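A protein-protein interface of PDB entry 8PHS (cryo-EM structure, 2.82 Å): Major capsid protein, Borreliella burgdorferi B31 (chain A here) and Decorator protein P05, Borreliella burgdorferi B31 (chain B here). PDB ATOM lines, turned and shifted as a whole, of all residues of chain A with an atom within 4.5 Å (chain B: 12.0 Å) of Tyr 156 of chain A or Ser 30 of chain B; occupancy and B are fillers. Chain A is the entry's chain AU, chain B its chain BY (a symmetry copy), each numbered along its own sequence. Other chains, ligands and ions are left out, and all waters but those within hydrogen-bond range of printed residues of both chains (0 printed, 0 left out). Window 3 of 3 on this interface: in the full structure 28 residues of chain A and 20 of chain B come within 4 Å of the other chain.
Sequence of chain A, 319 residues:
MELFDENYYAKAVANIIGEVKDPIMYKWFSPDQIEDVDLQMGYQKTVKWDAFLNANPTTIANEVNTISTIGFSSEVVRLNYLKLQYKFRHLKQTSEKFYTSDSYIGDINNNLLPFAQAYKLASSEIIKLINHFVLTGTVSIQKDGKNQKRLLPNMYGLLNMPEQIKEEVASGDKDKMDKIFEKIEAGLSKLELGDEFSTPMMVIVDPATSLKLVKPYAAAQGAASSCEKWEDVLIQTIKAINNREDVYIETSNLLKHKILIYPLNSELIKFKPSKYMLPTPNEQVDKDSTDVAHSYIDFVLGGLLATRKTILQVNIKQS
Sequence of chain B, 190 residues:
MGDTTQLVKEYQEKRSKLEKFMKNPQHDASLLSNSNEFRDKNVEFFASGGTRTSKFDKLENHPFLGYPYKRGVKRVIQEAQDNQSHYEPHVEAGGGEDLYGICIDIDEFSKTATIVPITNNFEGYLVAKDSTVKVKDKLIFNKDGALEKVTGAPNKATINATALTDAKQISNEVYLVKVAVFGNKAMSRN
The backbone carbonyl oxygen (O) of Ala 29 of chain B is in hydrogen-bond range of the side-chain amide nitrogen (ND2) of Asn 154 of chain A (3.4 Å).
The backbone carbonyl oxygen (O) of Asp 28 of chain B lies within hydrogen-bond range of the side-chain amide nitrogen (ND2) of Asn 154 of chain A (3.5 Å).
Among the printed residues, pairs that only touch across the chains: Val 77 of chain A with Ala 29 of chain B (3.5 Å), Val 77 of chain A with Leu 31 of chain B (3.9 Å), Val 77 of chain A with Leu 32 of chain B (3.6 Å), Asn 154 of chain A with Ser 30 of chain B (3.8 Å), Tyr 156 of chain A with Ser 30 of chain B (3.6 Å), Pro 162 of chain A with Ser 30 of chain B (3.7 Å) and Pro 162 of chain A with Leu 31 of chain B (3.3 Å).
Of chain B, only Ala 29, Leu 31 and Leu 32 come within 4 Å of Val 77 of chain A.
Tyr 156 of chain A touches just one residue of chain B: Ser 30 (3.6 Å).
No residue of chain B comes within 4 Å of Met 161 of chain A.
Pro 162 of chain A touches just these residues of chain B: Ser 30 (3.7 Å) and Leu 31 (3.3 Å).
Of the printed residues of chain A, Asp 28 of chain B touches Asn 154 (3.5 Å).
Of the printed residues of chain A, Ala 29 of chain B touches Val 77 (3.5 Å) and Asn 154 (3.4 Å).
Ser 30 of chain B touches just these residues of chain A: Asn 154, Tyr 156 and Pro 162.
Printed residues of chain A within 4 Å of Leu 31 of chain B: Val 77 and Pro 162.
Printed residues of chain A within 4 Å of Leu 32 of chain B: Val 77.
Ser 33 of chain B touches none of the printed residues of chain A.
The nearest residue of chain B that does not touch Tyr 156 of chain A is Leu 31 of chain B (6.1 Å).
The nearest residue of chain A that does not touch Ser 30 of chain B is Val 77 of chain A (4.1 Å).
The nearest printed residue of chain A that does not touch Ala 29 of chain B is Tyr 156 of chain A (6.9 Å).
Of the 10 printed residues of chain A, 4 touch a printed residue of chain B.
Printed residues of chain A that touch a printed residue of chain B: Val 77, Asn 154, Tyr 156 and Pro 162.
Hydrophobic or aromatic side chains of chain A within 4 Å of the printed part of chain B: Val 77, Tyr 156 and Pro 162.
Printed residues of chain B that touch a printed residue of chain A: Asp 28, Ala 29, Ser 30, Leu 31 and Leu 32.
Hydrophobic or aromatic side chains of chain B that line the printed part of chain A: Leu 31 and Leu 32.
Among the printed residues, no Asp or Glu carboxylate lies within 4 Å of a Lys or Arg side-chain nitrogen of the other chain.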
ATOM      1  N   VAL A  77      -2.236   1.646 -23.497  1.00  0.00           N
ATOM      2  CA  VAL A  77      -0.968   0.993 -23.206  1.00  0.00           C
ATOM      3  C   VAL A  77      -0.209   0.835 -24.513  1.00  0.00           C
ATOM      4  O   VAL A  77      -0.727   0.255 -25.477  1.00  0.00           O
ATOM      5  CB  VAL A  77      -1.184  -0.364 -22.517  1.00  0.00           C
ATOM      6  CG1 VAL A  77       0.148  -1.039 -22.271  1.00  0.00           C
ATOM      7  CG2 VAL A  77      -1.936  -0.172 -21.212  1.00  0.00           C
ATOM      8  N   GLY A 137      16.019  -5.357 -18.379  1.00  0.00           N
ATOM      9  CA  GLY A 137      15.429  -4.126 -18.858  1.00  0.00           C
ATOM     10  C   GLY A 137      16.409  -3.053 -19.275  1.00  0.00           C
ATOM     11  O   GLY A 137      15.981  -1.934 -19.580  1.00  0.00           O
ATOM     12  N   ASN A 154       8.454   2.997 -22.414  1.00  0.00           N
ATOM     13  CA  ASN A 154       7.656   1.774 -22.510  1.00  0.00           C
ATOM     14  C   ASN A 154       8.477   0.620 -23.081  1.00  0.00           C
ATOM     15  O   ASN A 154       7.999  -0.162 -23.903  1.00  0.00           O
ATOM     16  CB  ASN A 154       6.385   1.996 -23.332  1.00  0.00           C
ATOM     17  CG  ASN A 154       5.539   3.132 -22.798  1.00  0.00           C
ATOM     18  OD1 ASN A 154       5.914   3.803 -21.838  1.00  0.00           O
ATOM     19  ND2 ASN A 154       4.388   3.353 -23.419  1.00  0.00           N
ATOM     20  N   MET A 155       9.729   0.518 -22.641  1.00  0.00           N
ATOM     21  CA  MET A 155      10.614  -0.591 -22.994  1.00  0.00           C
ATOM     22  C   MET A 155      11.239  -1.084 -21.694  1.00  0.00           C
ATOM     23  O   MET A 155      12.210  -0.501 -21.204  1.00  0.00           O
ATOM     24  CB  MET A 155      11.674  -0.160 -24.000  1.00  0.00           C
ATOM     25  CG  MET A 155      11.141   0.050 -25.406  1.00  0.00           C
ATOM     26  SD  MET A 155      12.406   0.608 -26.559  1.00  0.00           S
ATOM     27  CE  MET A 155      13.050  -0.963 -27.125  1.00  0.00           C
ATOM     28  N   TYR A 156      10.681  -2.156 -21.138  1.00  0.00           N
ATOM     29  CA  TYR A 156      11.049  -2.622 -19.811  1.00  0.00           C
ATOM     30  C   TYR A 156      11.299  -4.122 -19.828  1.00  0.00           C
ATOM     31  O   TYR A 156      10.828  -4.846 -20.708  1.00  0.00           O
ATOM     32  CB  TYR A 156       9.957  -2.297 -18.785  1.00  0.00           C
ATOM     33  CG  TYR A 156       9.702  -0.820 -18.602  1.00  0.00           C
ATOM     34  CD1 TYR A 156      10.667   0.007 -18.048  1.00  0.00           C
ATOM     35  CD2 TYR A 156       8.495  -0.254 -18.987  1.00  0.00           C
ATOM     36  CE1 TYR A 156      10.438   1.357 -17.880  1.00  0.00           C
ATOM     37  CE2 TYR A 156       8.257   1.094 -18.824  1.00  0.00           C
ATOM     38  CZ  TYR A 156       9.231   1.895 -18.270  1.00  0.00           C
ATOM     39  OH  TYR A 156       8.999   3.241 -18.104  1.00  0.00           O
ATOM     40  N   GLY A 157      12.058  -4.579 -18.833  1.00  0.00           N
ATOM     41  CA  GLY A 157      12.275  -5.985 -18.592  1.00  0.00           C
ATOM     42  C   GLY A 157      11.572  -6.446 -17.324  1.00  0.00           C
ATOM     43  O   GLY A 157      10.891  -5.690 -16.637  1.00  0.00           O
ATOM     44  N   ASN A 160      12.961  -4.441 -14.133  1.00  0.00           N
ATOM     45  CA  ASN A 160      12.751  -3.005 -13.974  1.00  0.00           C
ATOM     46  C   ASN A 160      11.338  -2.574 -14.346  1.00  0.00           C
ATOM     47  O   ASN A 160      11.099  -1.384 -14.571  1.00  0.00           O
ATOM     48  CB  ASN A 160      13.771  -2.216 -14.798  1.00  0.00           C
ATOM     49  CG  ASN A 160      13.603  -2.421 -16.292  1.00  0.00           C
ATOM     50  OD1 ASN A 160      12.918  -3.343 -16.734  1.00  0.00           O
ATOM     51  ND2 ASN A 160      14.226  -1.552 -17.078  1.00  0.00           N
ATOM     52  N   MET A 161      10.398  -3.509 -14.421  1.00  0.00           N
ATOM     53  CA  MET A 161       9.026  -3.147 -14.736  1.00  0.00           C
ATOM     54  C   MET A 161       8.452  -2.278 -13.622  1.00  0.00           C
ATOM     55  O   MET A 161       8.522  -2.661 -12.446  1.00  0.00           O
ATOM     56  CB  MET A 161       8.170  -4.399 -14.925  1.00  0.00           C
ATOM     57  CG  MET A 161       6.804  -4.128 -15.529  1.00  0.00           C
ATOM     58  SD  MET A 161       6.881  -3.628 -17.257  1.00  0.00           S
ATOM     59  CE  MET A 161       6.986  -5.223 -18.063  1.00  0.00           C
ATOM     60  N   PRO A 162       7.890  -1.118 -13.937  1.00  0.00           N
ATOM     61  CA  PRO A 162       7.362  -0.234 -12.896  1.00  0.00           C
ATOM     62  C   PRO A 162       6.031  -0.742 -12.358  1.00  0.00           C
ATOM     63  O   PRO A 162       5.392  -1.629 -12.925  1.00  0.00           O
ATOM     64  CB  PRO A 162       7.196   1.101 -13.624  1.00  0.00           C
ATOM     65  CG  PRO A 162       6.921   0.708 -15.031  1.00  0.00           C
ATOM     66  CD  PRO A 162       7.718  -0.547 -15.285  1.00  0.00           C
ATOM     67  N   LEU A 304       7.554  -6.330 -23.937  1.00  0.00           N
ATOM     68  CA  LEU A 304       7.143  -6.970 -22.694  1.00  0.00           C
ATOM     69  C   LEU A 304       5.949  -6.229 -22.104  1.00  0.00           C
ATOM     70  O   LEU A 304       6.006  -5.011 -21.909  1.00  0.00           O
ATOM     71  CB  LEU A 304       8.293  -7.009 -21.687  1.00  0.00           C
ATOM     72  CG  LEU A 304       8.078  -7.964 -20.511  1.00  0.00           C
ATOM     73  CD1 LEU A 304       7.952  -9.398 -20.999  1.00  0.00           C
ATOM     74  CD2 LEU A 304       9.202  -7.838 -19.503  1.00  0.00           C
ATOM     75  N   ASN B  24      -6.120  14.022 -19.925  1.00  0.00           N
ATOM     76  CA  ASN B  24      -5.905  12.599 -19.665  1.00  0.00           C
ATOM     77  C   ASN B  24      -4.433  12.279 -19.884  1.00  0.00           C
ATOM     78  O   ASN B  24      -4.019  11.956 -21.008  1.00  0.00           O
ATOM     79  CB  ASN B  24      -6.788  11.735 -20.561  1.00  0.00           C
ATOM     80  CG  ASN B  24      -8.265  11.938 -20.296  1.00  0.00           C
ATOM     81  OD1 ASN B  24      -8.651  12.690 -19.403  1.00  0.00           O
ATOM     82  ND2 ASN B  24      -9.102  11.269 -21.082  1.00  0.00           N
ATOM     83  N   PRO B  25      -3.607  12.352 -18.842  1.00  0.00           N
ATOM     84  CA  PRO B  25      -2.196  11.978 -18.970  1.00  0.00           C
ATOM     85  C   PRO B  25      -1.922  10.492 -18.808  1.00  0.00           C
ATOM     86  O   PRO B  25      -0.759  10.083 -18.895  1.00  0.00           O
ATOM     87  CB  PRO B  25      -1.552  12.774 -17.831  1.00  0.00           C
ATOM     88  CG  PRO B  25      -2.595  12.760 -16.761  1.00  0.00           C
ATOM     89  CD  PRO B  25      -3.941  12.760 -17.464  1.00  0.00           C
ATOM     90  N   GLN B  26      -2.957   9.683 -18.580  1.00  0.00           N
ATOM     91  CA  GLN B  26      -2.789   8.245 -18.423  1.00  0.00           C
ATOM     92  C   GLN B  26      -2.645   7.516 -19.752  1.00  0.00           C
ATOM     93  O   GLN B  26      -2.394   6.307 -19.749  1.00  0.00           O
ATOM     94  CB  GLN B  26      -3.969   7.664 -17.642  1.00  0.00           C
ATOM     95  CG  GLN B  26      -4.210   8.349 -16.309  1.00  0.00           C
ATOM     96  CD  GLN B  26      -2.976   8.359 -15.431  1.00  0.00           C
ATOM     97  OE1 GLN B  26      -2.437   9.418 -15.113  1.00  0.00           O
ATOM     98  NE2 GLN B  26      -2.524   7.176 -15.031  1.00  0.00           N
ATOM     99  N   HIS B  27      -2.803   8.211 -20.874  1.00  0.00           N
ATOM    100  CA  HIS B  27      -2.578   7.596 -22.171  1.00  0.00           C
ATOM    101  C   HIS B  27      -1.089   7.344 -22.384  1.00  0.00           C
ATOM    102  O   HIS B  27      -0.228   7.956 -21.746  1.00  0.00           O
ATOM    103  CB  HIS B  27      -3.135   8.475 -23.289  1.00  0.00           C
ATOM    104  CG  HIS B  27      -4.597   8.758 -23.155  1.00  0.00           C
ATOM    105  ND1 HIS B  27      -5.534   7.762 -22.991  1.00  0.00           N
ATOM    106  CD2 HIS B  27      -5.285   9.924 -23.164  1.00  0.00           C
ATOM    107  CE1 HIS B  27      -6.736   8.302 -22.898  1.00  0.00           C
ATOM    108  NE2 HIS B  27      -6.614   9.613 -23.005  1.00  0.00           N
ATOM    109  N   ASP B  28      -0.794   6.424 -23.305  1.00  0.00           N
ATOM    110  CA  ASP B  28       0.567   5.926 -23.513  1.00  0.00           C
ATOM    111  C   ASP B  28       1.151   5.396 -22.206  1.00  0.00           C
ATOM    112  O   ASP B  28       2.300   5.672 -21.858  1.00  0.00           O
ATOM    113  CB  ASP B  28       1.469   7.000 -24.125  1.00  0.00           C
ATOM    114  CG  ASP B  28       0.999   7.439 -25.497  1.00  0.00           C
ATOM    115  OD1 ASP B  28      -0.053   6.943 -25.951  1.00  0.00           O
ATOM    116  OD2 ASP B  28       1.683   8.276 -26.123  1.00  0.00           O
ATOM    117  N   ALA B  29       0.342   4.636 -21.472  1.00  0.00           N
ATOM    118  CA  ALA B  29       0.779   4.067 -20.207  1.00  0.00           C
ATOM    119  C   ALA B  29       1.795   2.955 -20.440  1.00  0.00           C
ATOM    120  O   ALA B  29       1.821   2.315 -21.494  1.00  0.00           O
ATOM    121  CB  ALA B  29      -0.415   3.529 -19.420  1.00  0.00           C
ATOM    122  N   SER B  30       2.641   2.733 -19.435  1.00  0.00           N
ATOM    123  CA  SER B  30       3.712   1.753 -19.572  1.00  0.00           C
ATOM    124  C   SER B  30       3.200   0.321 -19.462  1.00  0.00           C
ATOM    125  O   SER B  30       3.675  -0.562 -20.184  1.00  0.00           O
ATOM    126  CB  SER B  30       4.795   2.021 -18.527  1.00  0.00           C
ATOM    127  OG  SER B  30       4.245   2.076 -17.225  1.00  0.00           O
ATOM    128  N   LEU B  31       2.238   0.064 -18.578  1.00  0.00           N
ATOM    129  CA  LEU B  31       1.783  -1.300 -18.344  1.00  0.00           C
ATOM    130  C   LEU B  31       0.299  -1.298 -18.004  1.00  0.00           C
ATOM    131  O   LEU B  31      -0.296  -0.258 -17.715  1.00  0.00           O
ATOM    132  CB  LEU B  31       2.580  -1.978 -17.224  1.00  0.00           C
ATOM    133  CG  LEU B  31       2.332  -1.558 -15.772  1.00  0.00           C
ATOM    134  CD1 LEU B  31       2.924  -2.593 -14.831  1.00  0.00           C
ATOM    135  CD2 LEU B  31       2.900  -0.184 -15.464  1.00  0.00           C
ATOM    136  N   LEU B  32      -0.290  -2.491 -18.043  1.00  0.00           N
ATOM    137  CA  LEU B  32      -1.680  -2.668 -17.646  1.00  0.00           C
ATOM    138  C   LEU B  32      -1.851  -2.393 -16.157  1.00  0.00           C
ATOM    139  O   LEU B  32      -0.956  -2.650 -15.348  1.00  0.00           O
ATOM    140  CB  LEU B  32      -2.150  -4.087 -17.968  1.00  0.00           C
ATOM    141  CG  LEU B  32      -2.122  -4.519 -19.434  1.00  0.00           C
ATOM    142  CD1 LEU B  32      -2.686  -5.919 -19.588  1.00  0.00           C
ATOM    143  CD2 LEU B  32      -2.902  -3.536 -20.287  1.00  0.00           C
ATOM    144  N   SER B  33      -3.018  -1.871 -15.796  1.00  0.00           N
ATOM    145  CA  SER B  33      -3.312  -1.484 -14.424  1.00  0.00           C
ATOM    146  C   SER B  33      -4.226  -2.511 -13.770  1.00  0.00           C
ATOM    147  O   SER B  33      -5.164  -3.014 -14.394  1.00  0.00           O
ATOM    148  CB  SER B  33      -3.962  -0.101 -14.375  1.00  0.00           C
ATOM    149  OG  SER B  33      -5.197  -0.094 -15.070  1.00  0.00           O
ATOM    150  N   ASN B  34      -3.942  -2.820 -12.506  1.00  0.00           N
ATOM    151  CA  ASN B  34      -4.753  -3.766 -11.755  1.00  0.00           C
ATOM    152  C   ASN B  34      -6.060  -3.113 -11.322  1.00  0.00           C
ATOM    153  O   ASN B  34      -6.081  -1.952 -10.903  1.00  0.00           O
ATOM    154  CB  ASN B  34      -3.988  -4.271 -10.533  1.00  0.00           C
ATOM    155  CG  ASN B  34      -4.614  -5.508  -9.927  1.00  0.00           C
ATOM    156  OD1 ASN B  34      -5.593  -6.039 -10.448  1.00  0.00           O
ATOM    157  ND2 ASN B  34      -4.052  -5.973  -8.820  1.00  0.00           N
